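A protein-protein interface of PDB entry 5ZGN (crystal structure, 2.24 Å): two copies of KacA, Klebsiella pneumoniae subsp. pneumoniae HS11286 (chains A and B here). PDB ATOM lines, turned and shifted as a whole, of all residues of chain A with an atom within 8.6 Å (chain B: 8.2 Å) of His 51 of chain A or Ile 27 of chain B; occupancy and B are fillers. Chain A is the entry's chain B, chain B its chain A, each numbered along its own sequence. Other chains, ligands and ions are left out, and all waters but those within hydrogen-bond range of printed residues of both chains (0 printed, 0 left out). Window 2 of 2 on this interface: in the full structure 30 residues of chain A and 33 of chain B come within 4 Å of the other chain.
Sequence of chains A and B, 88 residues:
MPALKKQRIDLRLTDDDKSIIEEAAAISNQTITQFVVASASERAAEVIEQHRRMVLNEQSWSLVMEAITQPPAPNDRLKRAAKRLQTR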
ATOM      1  N   ALA A  44      13.499   8.802  -0.083  1.00  0.00           N
ATOM      2  CA  ALA A  44      13.063   8.327   1.226  1.00  0.00           C
ATOM      3  C   ALA A  44      12.193   7.083   1.096  1.00  0.00           C
ATOM      4  O   ALA A  44      12.411   6.085   1.794  1.00  0.00           O
ATOM      5  CB  ALA A  44      12.309   9.438   1.959  1.00  0.00           C
ATOM      6  N   ALA A  45      11.202   7.124   0.201  1.00  0.00           N
ATOM      7  CA  ALA A  45      10.323   5.974   0.010  1.00  0.00           C
ATOM      8  C   ALA A  45      11.097   4.747  -0.452  1.00  0.00           C
ATOM      9  O   ALA A  45      10.735   3.618  -0.102  1.00  0.00           O
ATOM     10  CB  ALA A  45       9.218   6.315  -0.991  1.00  0.00           C
ATOM     11  N   GLU A  46      12.157   4.945  -1.236  1.00  0.00           N
ATOM     12  CA  GLU A  46      13.003   3.825  -1.638  1.00  0.00           C
ATOM     13  C   GLU A  46      13.744   3.245  -0.440  1.00  0.00           C
ATOM     14  O   GLU A  46      13.801   2.024  -0.264  1.00  0.00           O
ATOM     15  CB  GLU A  46      13.986   4.275  -2.719  1.00  0.00           C
ATOM     16  CG  GLU A  46      13.338   4.527  -4.074  1.00  0.00           C
ATOM     17  CD  GLU A  46      14.287   5.170  -5.068  1.00  0.00           C
ATOM     18  OE1 GLU A  46      13.807   5.692  -6.095  1.00  0.00           O
ATOM     19  OE2 GLU A  46      15.510   5.157  -4.819  1.00  0.00           O
ATOM     20  N   VAL A  47      14.324   4.115   0.391  1.00  0.00           N
ATOM     21  CA  VAL A  47      15.036   3.655   1.580  1.00  0.00           C
ATOM     22  C   VAL A  47      14.089   2.928   2.527  1.00  0.00           C
ATOM     23  O   VAL A  47      14.421   1.863   3.062  1.00  0.00           O
ATOM     24  CB  VAL A  47      15.731   4.841   2.273  1.00  0.00           C
ATOM     25  CG1 VAL A  47      16.260   4.428   3.638  1.00  0.00           C
ATOM     26  CG2 VAL A  47      16.855   5.382   1.398  1.00  0.00           C
ATOM     27  N   ILE A  48      12.891   3.478   2.735  1.00  0.00           N
ATOM     28  CA  ILE A  48      11.961   2.892   3.695  1.00  0.00           C
ATOM     29  C   ILE A  48      11.483   1.521   3.231  1.00  0.00           C
ATOM     30  O   ILE A  48      11.400   0.579   4.028  1.00  0.00           O
ATOM     31  CB  ILE A  48      10.780   3.848   3.943  1.00  0.00           C
ATOM     32  CG1 ILE A  48      11.260   5.119   4.650  1.00  0.00           C
ATOM     33  CG2 ILE A  48       9.685   3.157   4.744  1.00  0.00           C
ATOM     34  CD1 ILE A  48      10.195   6.182   4.784  1.00  0.00           C
ATOM     35  N   GLU A  49      11.176   1.373   1.940  1.00  0.00           N
ATOM     36  CA  GLU A  49      10.638   0.096   1.475  1.00  0.00           C
ATOM     37  C   GLU A  49      11.719  -0.977   1.420  1.00  0.00           C
ATOM     38  O   GLU A  49      11.452  -2.150   1.703  1.00  0.00           O
ATOM     39  CB  GLU A  49       9.957   0.265   0.115  1.00  0.00           C
ATOM     40  CG  GLU A  49       9.104  -0.935  -0.293  1.00  0.00           C
ATOM     41  CD  GLU A  49       7.628  -0.746   0.027  1.00  0.00           C
ATOM     42  OE1 GLU A  49       7.320  -0.334   1.164  1.00  0.00           O
ATOM     43  OE2 GLU A  49       6.781  -1.026  -0.846  1.00  0.00           O
ATOM     44  N   GLN A  50      12.953  -0.599   1.074  1.00  0.00           N
ATOM     45  CA  GLN A  50      14.052  -1.553   1.160  1.00  0.00           C
ATOM     46  C   GLN A  50      14.323  -1.954   2.605  1.00  0.00           C
ATOM     47  O   GLN A  50      14.844  -3.047   2.863  1.00  0.00           O
ATOM     48  CB  GLN A  50      15.312  -0.964   0.525  1.00  0.00           C
ATOM     49  CG  GLN A  50      16.504  -1.905   0.515  1.00  0.00           C
ATOM     50  CD  GLN A  50      17.720  -1.315   1.200  1.00  0.00           C
ATOM     51  OE1 GLN A  50      18.213  -0.256   0.812  1.00  0.00           O
ATOM     52  NE2 GLN A  50      18.208  -1.998   2.230  1.00  0.00           N
ATOM     53  N   HIS A  51      13.963  -1.093   3.558  1.00  0.00           N
ATOM     54  CA  HIS A  51      14.214  -1.377   4.964  1.00  0.00           C
ATOM     55  C   HIS A  51      13.197  -2.348   5.551  1.00  0.00           C
ATOM     56  O   HIS A  51      13.532  -3.105   6.468  1.00  0.00           O
ATOM     57  CB  HIS A  51      14.217  -0.074   5.765  1.00  0.00           C
ATOM     58  CG  HIS A  51      14.528  -0.258   7.217  1.00  0.00           C
ATOM     59  ND1 HIS A  51      13.567  -0.162   8.200  1.00  0.00           N
ATOM     60  CD2 HIS A  51      15.690  -0.536   7.852  1.00  0.00           C
ATOM     61  CE1 HIS A  51      14.124  -0.371   9.380  1.00  0.00           C
ATOM     62  NE2 HIS A  51      15.412  -0.601   9.197  1.00  0.00           N
ATOM     63  N   ARG A  52      11.960  -2.349   5.049  1.00  0.00           N
ATOM     64  CA  ARG A  52      10.928  -3.214   5.604  1.00  0.00           C
ATOM     65  C   ARG A  52      10.672  -4.477   4.789  1.00  0.00           C
ATOM     66  O   ARG A  52      10.042  -5.405   5.304  1.00  0.00           O
ATOM     67  CB  ARG A  52       9.614  -2.441   5.786  1.00  0.00           C
ATOM     68  CG  ARG A  52       9.132  -1.657   4.584  1.00  0.00           C
ATOM     69  CD  ARG A  52       8.041  -0.680   5.007  1.00  0.00           C
ATOM     70  NE  ARG A  52       7.484   0.061   3.880  1.00  0.00           N
ATOM     71  CZ  ARG A  52       6.606   1.052   4.001  1.00  0.00           C
ATOM     72  NH1 ARG A  52       6.188   1.426   5.204  1.00  0.00           N
ATOM     73  NH2 ARG A  52       6.149   1.671   2.921  1.00  0.00           N
ATOM     74  N   ARG A  53      11.109  -4.509   3.536  1.00  0.00           N
ATOM     75  CA  ARG A  53      10.858  -5.674   2.694  1.00  0.00           C
ATOM     76  C   ARG A  53      12.050  -6.615   2.578  1.00  0.00           C
ATOM     77  O   ARG A  53      13.086  -6.249   2.024  1.00  0.00           O
ATOM     78  CB  ARG A  53      10.405  -5.233   1.299  1.00  0.00           C
ATOM     79  CG  ARG A  53       8.903  -5.310   1.080  1.00  0.00           C
ATOM     80  CD  ARG A  53       8.494  -4.602  -0.201  1.00  0.00           C
ATOM     81  NE  ARG A  53       8.621  -5.469  -1.369  1.00  0.00           N
ATOM     82  CZ  ARG A  53       8.171  -5.160  -2.581  1.00  0.00           C
ATOM     83  NH1 ARG A  53       8.330  -6.010  -3.586  1.00  0.00           N
ATOM     84  NH2 ARG A  53       7.561  -4.002  -2.788  1.00  0.00           N
ATOM     85  N   MET A  54      11.900  -7.829   3.100  1.00  0.00           N
ATOM     86  CA  MET A  54      12.973  -8.818   3.030  1.00  0.00           C
ATOM     87  C   MET A  54      12.705  -9.815   1.910  1.00  0.00           C
ATOM     88  O   MET A  54      11.881 -10.717   2.055  1.00  0.00           O
ATOM     89  CB  MET A  54      13.135  -9.576   4.353  1.00  0.00           C
ATOM     90  CG  MET A  54      12.480  -8.941   5.569  1.00  0.00           C
ATOM     91  SD  MET A  54      13.776  -8.360   6.904  1.00  0.00           S
ATOM     92  CE  MET A  54      14.274  -6.656   6.089  1.00  0.00           C
ATOM     93  N   ILE B  20       8.801  11.296   6.622  1.00  0.00           N
ATOM     94  CA  ILE B  20       9.413  10.238   5.824  1.00  0.00           C
ATOM     95  C   ILE B  20      10.847  10.595   5.457  1.00  0.00           C
ATOM     96  O   ILE B  20      11.692   9.705   5.306  1.00  0.00           O
ATOM     97  CB  ILE B  20       8.572   9.941   4.568  1.00  0.00           C
ATOM     98  CG1 ILE B  20       8.627  11.113   3.586  1.00  0.00           C
ATOM     99  CG2 ILE B  20       7.136   9.622   4.950  1.00  0.00           C
ATOM    100  CD1 ILE B  20       8.313  10.734   2.156  1.00  0.00           C
ATOM    101  N   ILE B  21      11.153  11.887   5.311  1.00  0.00           N
ATOM    102  CA  ILE B  21      12.529  12.289   5.039  1.00  0.00           C
ATOM    103  C   ILE B  21      13.384  12.150   6.294  1.00  0.00           C
ATOM    104  O   ILE B  21      14.514  11.649   6.239  1.00  0.00           O
ATOM    105  CB  ILE B  21      12.568  13.722   4.474  1.00  0.00           C
ATOM    106  CG1 ILE B  21      12.065  13.739   3.027  1.00  0.00           C
ATOM    107  CG2 ILE B  21      13.973  14.302   4.563  1.00  0.00           C
ATOM    108  CD1 ILE B  21      11.807  15.128   2.486  1.00  0.00           C
ATOM    109  N   GLU B  22      12.857  12.582   7.443  1.00  0.00           N
ATOM    110  CA  GLU B  22      13.588  12.449   8.701  1.00  0.00           C
ATOM    111  C   GLU B  22      13.902  10.990   9.009  1.00  0.00           C
ATOM    112  O   GLU B  22      15.037  10.645   9.360  1.00  0.00           O
ATOM    113  CB  GLU B  22      12.784  13.065   9.846  1.00  0.00           C
ATOM    114  CG  GLU B  22      12.917  14.567   9.992  1.00  0.00           C
ATOM    115  CD  GLU B  22      12.077  15.108  11.134  1.00  0.00           C
ATOM    116  OE1 GLU B  22      11.128  14.413  11.556  1.00  0.00           O
ATOM    117  OE2 GLU B  22      12.377  16.218  11.621  1.00  0.00           O
ATOM    118  N   GLU B  23      12.903  10.114   8.885  1.00  0.00           N
ATOM    119  CA  GLU B  23      13.090   8.728   9.292  1.00  0.00           C
ATOM    120  C   GLU B  23      13.908   7.935   8.281  1.00  0.00           C
ATOM    121  O   GLU B  23      14.624   7.005   8.669  1.00  0.00           O
ATOM    122  CB  GLU B  23      11.730   8.067   9.521  1.00  0.00           C
ATOM    123  CG  GLU B  23      10.963   8.665  10.695  1.00  0.00           C
ATOM    124  CD  GLU B  23       9.896   7.737  11.240  1.00  0.00           C
ATOM    125  OE1 GLU B  23       8.810   8.229  11.612  1.00  0.00           O
ATOM    126  OE2 GLU B  23      10.139   6.514  11.285  1.00  0.00           O
ATOM    127  N   ALA B  24      13.824   8.283   6.994  1.00  0.00           N
ATOM    128  CA  ALA B  24      14.701   7.655   6.011  1.00  0.00           C
ATOM    129  C   ALA B  24      16.147   8.076   6.220  1.00  0.00           C
ATOM    130  O   ALA B  24      17.068   7.271   6.034  1.00  0.00           O
ATOM    131  CB  ALA B  24      14.246   7.999   4.595  1.00  0.00           C
ATOM    132  N   ALA B  25      16.368   9.338   6.595  1.00  0.00           N
ATOM    133  CA  ALA B  25      17.709   9.772   6.967  1.00  0.00           C
ATOM    134  C   ALA B  25      18.182   9.059   8.227  1.00  0.00           C
ATOM    135  O   ALA B  25      19.370   8.748   8.367  1.00  0.00           O
ATOM    136  CB  ALA B  25      17.737  11.288   7.158  1.00  0.00           C
ATOM    137  N   ALA B  26      17.263   8.795   9.160  1.00  0.00           N
ATOM    138  CA  ALA B  26      17.620   8.033  10.352  1.00  0.00           C
ATOM    139  C   ALA B  26      18.000   6.602   9.996  1.00  0.00           C
ATOM    140  O   ALA B  26      18.975   6.062  10.533  1.00  0.00           O
ATOM    141  CB  ALA B  26      16.467   8.053  11.356  1.00  0.00           C
ATOM    142  N   ILE B  27      17.242   5.971   9.095  1.00  0.00           N
ATOM    143  CA  ILE B  27      17.585   4.625   8.643  1.00  0.00           C
ATOM    144  C   ILE B  27      18.949   4.625   7.964  1.00  0.00           C
ATOM    145  O   ILE B  27      19.788   3.753   8.221  1.00  0.00           O
ATOM    146  CB  ILE B  27      16.485   4.079   7.711  1.00  0.00           C
ATOM    147  CG1 ILE B  27      15.191   3.845   8.491  1.00  0.00           C
ATOM    148  CG2 ILE B  27      16.940   2.794   7.028  1.00  0.00           C
ATOM    149  CD1 ILE B  27      13.991   3.574   7.610  1.00  0.00           C
ATOM    150  N   SER B  28      19.199   5.610   7.097  1.00  0.00           N
ATOM    151  CA  SER B  28      20.487   5.718   6.423  1.00  0.00           C
ATOM    152  C   SER B  28      21.593   6.230   7.338  1.00  0.00           C
ATOM    153  O   SER B  28      22.752   6.261   6.914  1.00  0.00           O
ATOM    154  CB  SER B  28      20.363   6.640   5.207  1.00  0.00           C
ATOM    155  OG  SER B  28      19.244   6.290   4.411  1.00  0.00           O
ATOM    156  N   ASN B  29      21.264   6.614   8.572  1.00  0.00           N
ATOM    157  CA  ASN B  29      22.220   7.190   9.520  1.00  0.00           C
ATOM    158  C   ASN B  29      22.965   8.375   8.902  1.00  0.00           C
ATOM    159  O   ASN B  29      24.191   8.482   8.969  1.00  0.00           O
ATOM    160  CB  ASN B  29      23.196   6.130  10.032  1.00  0.00           C
ATOM    161  CG  ASN B  29      23.806   6.498  11.375  1.00  0.00           C
ATOM    162  OD1 ASN B  29      23.328   7.405  12.058  1.00  0.00           O
ATOM    163  ND2 ASN B  29      24.863   5.792  11.759  1.00  0.00           N
ATOM    164  N   GLN B  30      22.198   9.272   8.287  1.00  0.00           N
ATOM    165  CA  GLN B  30      22.716  10.515   7.735  1.00  0.00           C
ATOM    166  C   GLN B  30      21.911  11.672   8.308  1.00  0.00           C
ATOM    167  O   GLN B  30      20.709  11.543   8.553  1.00  0.00           O
ATOM    168  CB  GLN B  30      22.633  10.526   6.194  1.00  0.00           C
ATOM    169  CG  GLN B  30      23.277   9.321   5.511  1.00  0.00           C
ATOM    170  CD  GLN B  30      23.100   9.336   3.999  1.00  0.00           C
ATOM    171  OE1 GLN B  30      22.443  10.218   3.448  1.00  0.00           O
ATOM    172  NE2 GLN B  30      23.689   8.354   3.324  1.00  0.00           N
ATOM    173  N   PHE B  35      21.209  13.681   3.603  1.00  0.00           N
ATOM    174  CA  PHE B  35      20.189  12.936   2.872  1.00  0.00           C
ATOM    175  C   PHE B  35      19.480  13.813   1.842  1.00  0.00           C
ATOM    176  O   PHE B  35      19.239  13.379   0.712  1.00  0.00           O
ATOM    177  CB  PHE B  35      19.179  12.333   3.849  1.00  0.00           C
ATOM    178  CG  PHE B  35      18.209  11.384   3.203  1.00  0.00           C
ATOM    179  CD1 PHE B  35      17.025  11.845   2.647  1.00  0.00           C
ATOM    180  CD2 PHE B  35      18.486  10.027   3.147  1.00  0.00           C
ATOM    181  CE1 PHE B  35      16.136  10.971   2.048  1.00  0.00           C
ATOM    182  CE2 PHE B  35      17.602   9.148   2.552  1.00  0.00           C
ATOM    183  CZ  PHE B  35      16.425   9.620   2.002  1.00  0.00           C
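O of Ala 24 of chain B lies within hydrogen-bond range of OG of Ser 28 of chain B (2.9 Å).
Ile 20 of chain B touches Ala 44 of chain A (O to CB, 3.4 Å).
Ala 44 of chain A touches Ala 24 of chain B (CB to CB, 3.6 Å).
Ala 44 of chain A touches Phe 35 of chain B (CA to CZ, 3.7 Å).
Ala 24 of chain B touches Val 47 of chain A (O to CG1, 3.8 Å).
Val 47 of chain A touches Ile 27 of chain B (CG1 to CG2, 3.8 Å).
Ser 28 of chain B touches Val 47 of chain A.
CD1 of Ile 48 of chain A touches O of Ile 20 of chain B, at 3.9 Å.
His 51 of chain A touches Ile 27 of chain B.
Of the printed residues of chain B, Ala 44 of chain A touches Ile 20 (3.4 Å), Ala 24 (3.6 Å) and Phe 35 (3.7 Å).
Ala 45 of chain A touches none of the printed residues of chain B.
His 51 of chain A touches just one residue of chain B: Ile 27.
Printed residues of chain A within 4 Å of Ile 20 of chain B: Ala 44 (3.4 Å) and Ile 48 (3.9 Å).
Glu 23 of chain B touches none of the printed residues of chain A.
Printed residues of chain A within 4 Å of Ala 24 of chain B: Ala 44 and Val 47.
No residue of chain A comes within 4 Å of Ala 26 of chain B.
Of chain A, only Val 47 (3.8 Å) and His 51 (3.7 Å) come within 4 Å of Ile 27 of chain B.
Ser 28 of chain B touches just one residue of chain A: Val 47 (3.6 Å).
Printed residues of chain A within 4 Å of Phe 35 of chain B: Ala 44 (3.7 Å).
The nearest residue of chain A that does not touch Ile 27 of chain B is Ile 48 of chain A (4.3 Å).
Printed residues of chain B that touch a printed residue of chain A: Ile 20, Ala 24, Ile 27, Ser 28 and Phe 35.
Hydrophobic or aromatic side chains of chain B within 4 Å of the printed part of chain A: Ala 24, Ile 27 and Phe 35.
Of the 11 printed residues of chain A, 4 touch a printed residue of chain B.
Along chain A the printed residues that touch a printed residue of chain B span positions 44 to 51.
Among the printed residues, no Asp or Glu carboxylate lies within 4 Å of a Lys or Arg side-chain nitrogen of the other chain.
No position is printed for both chains.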
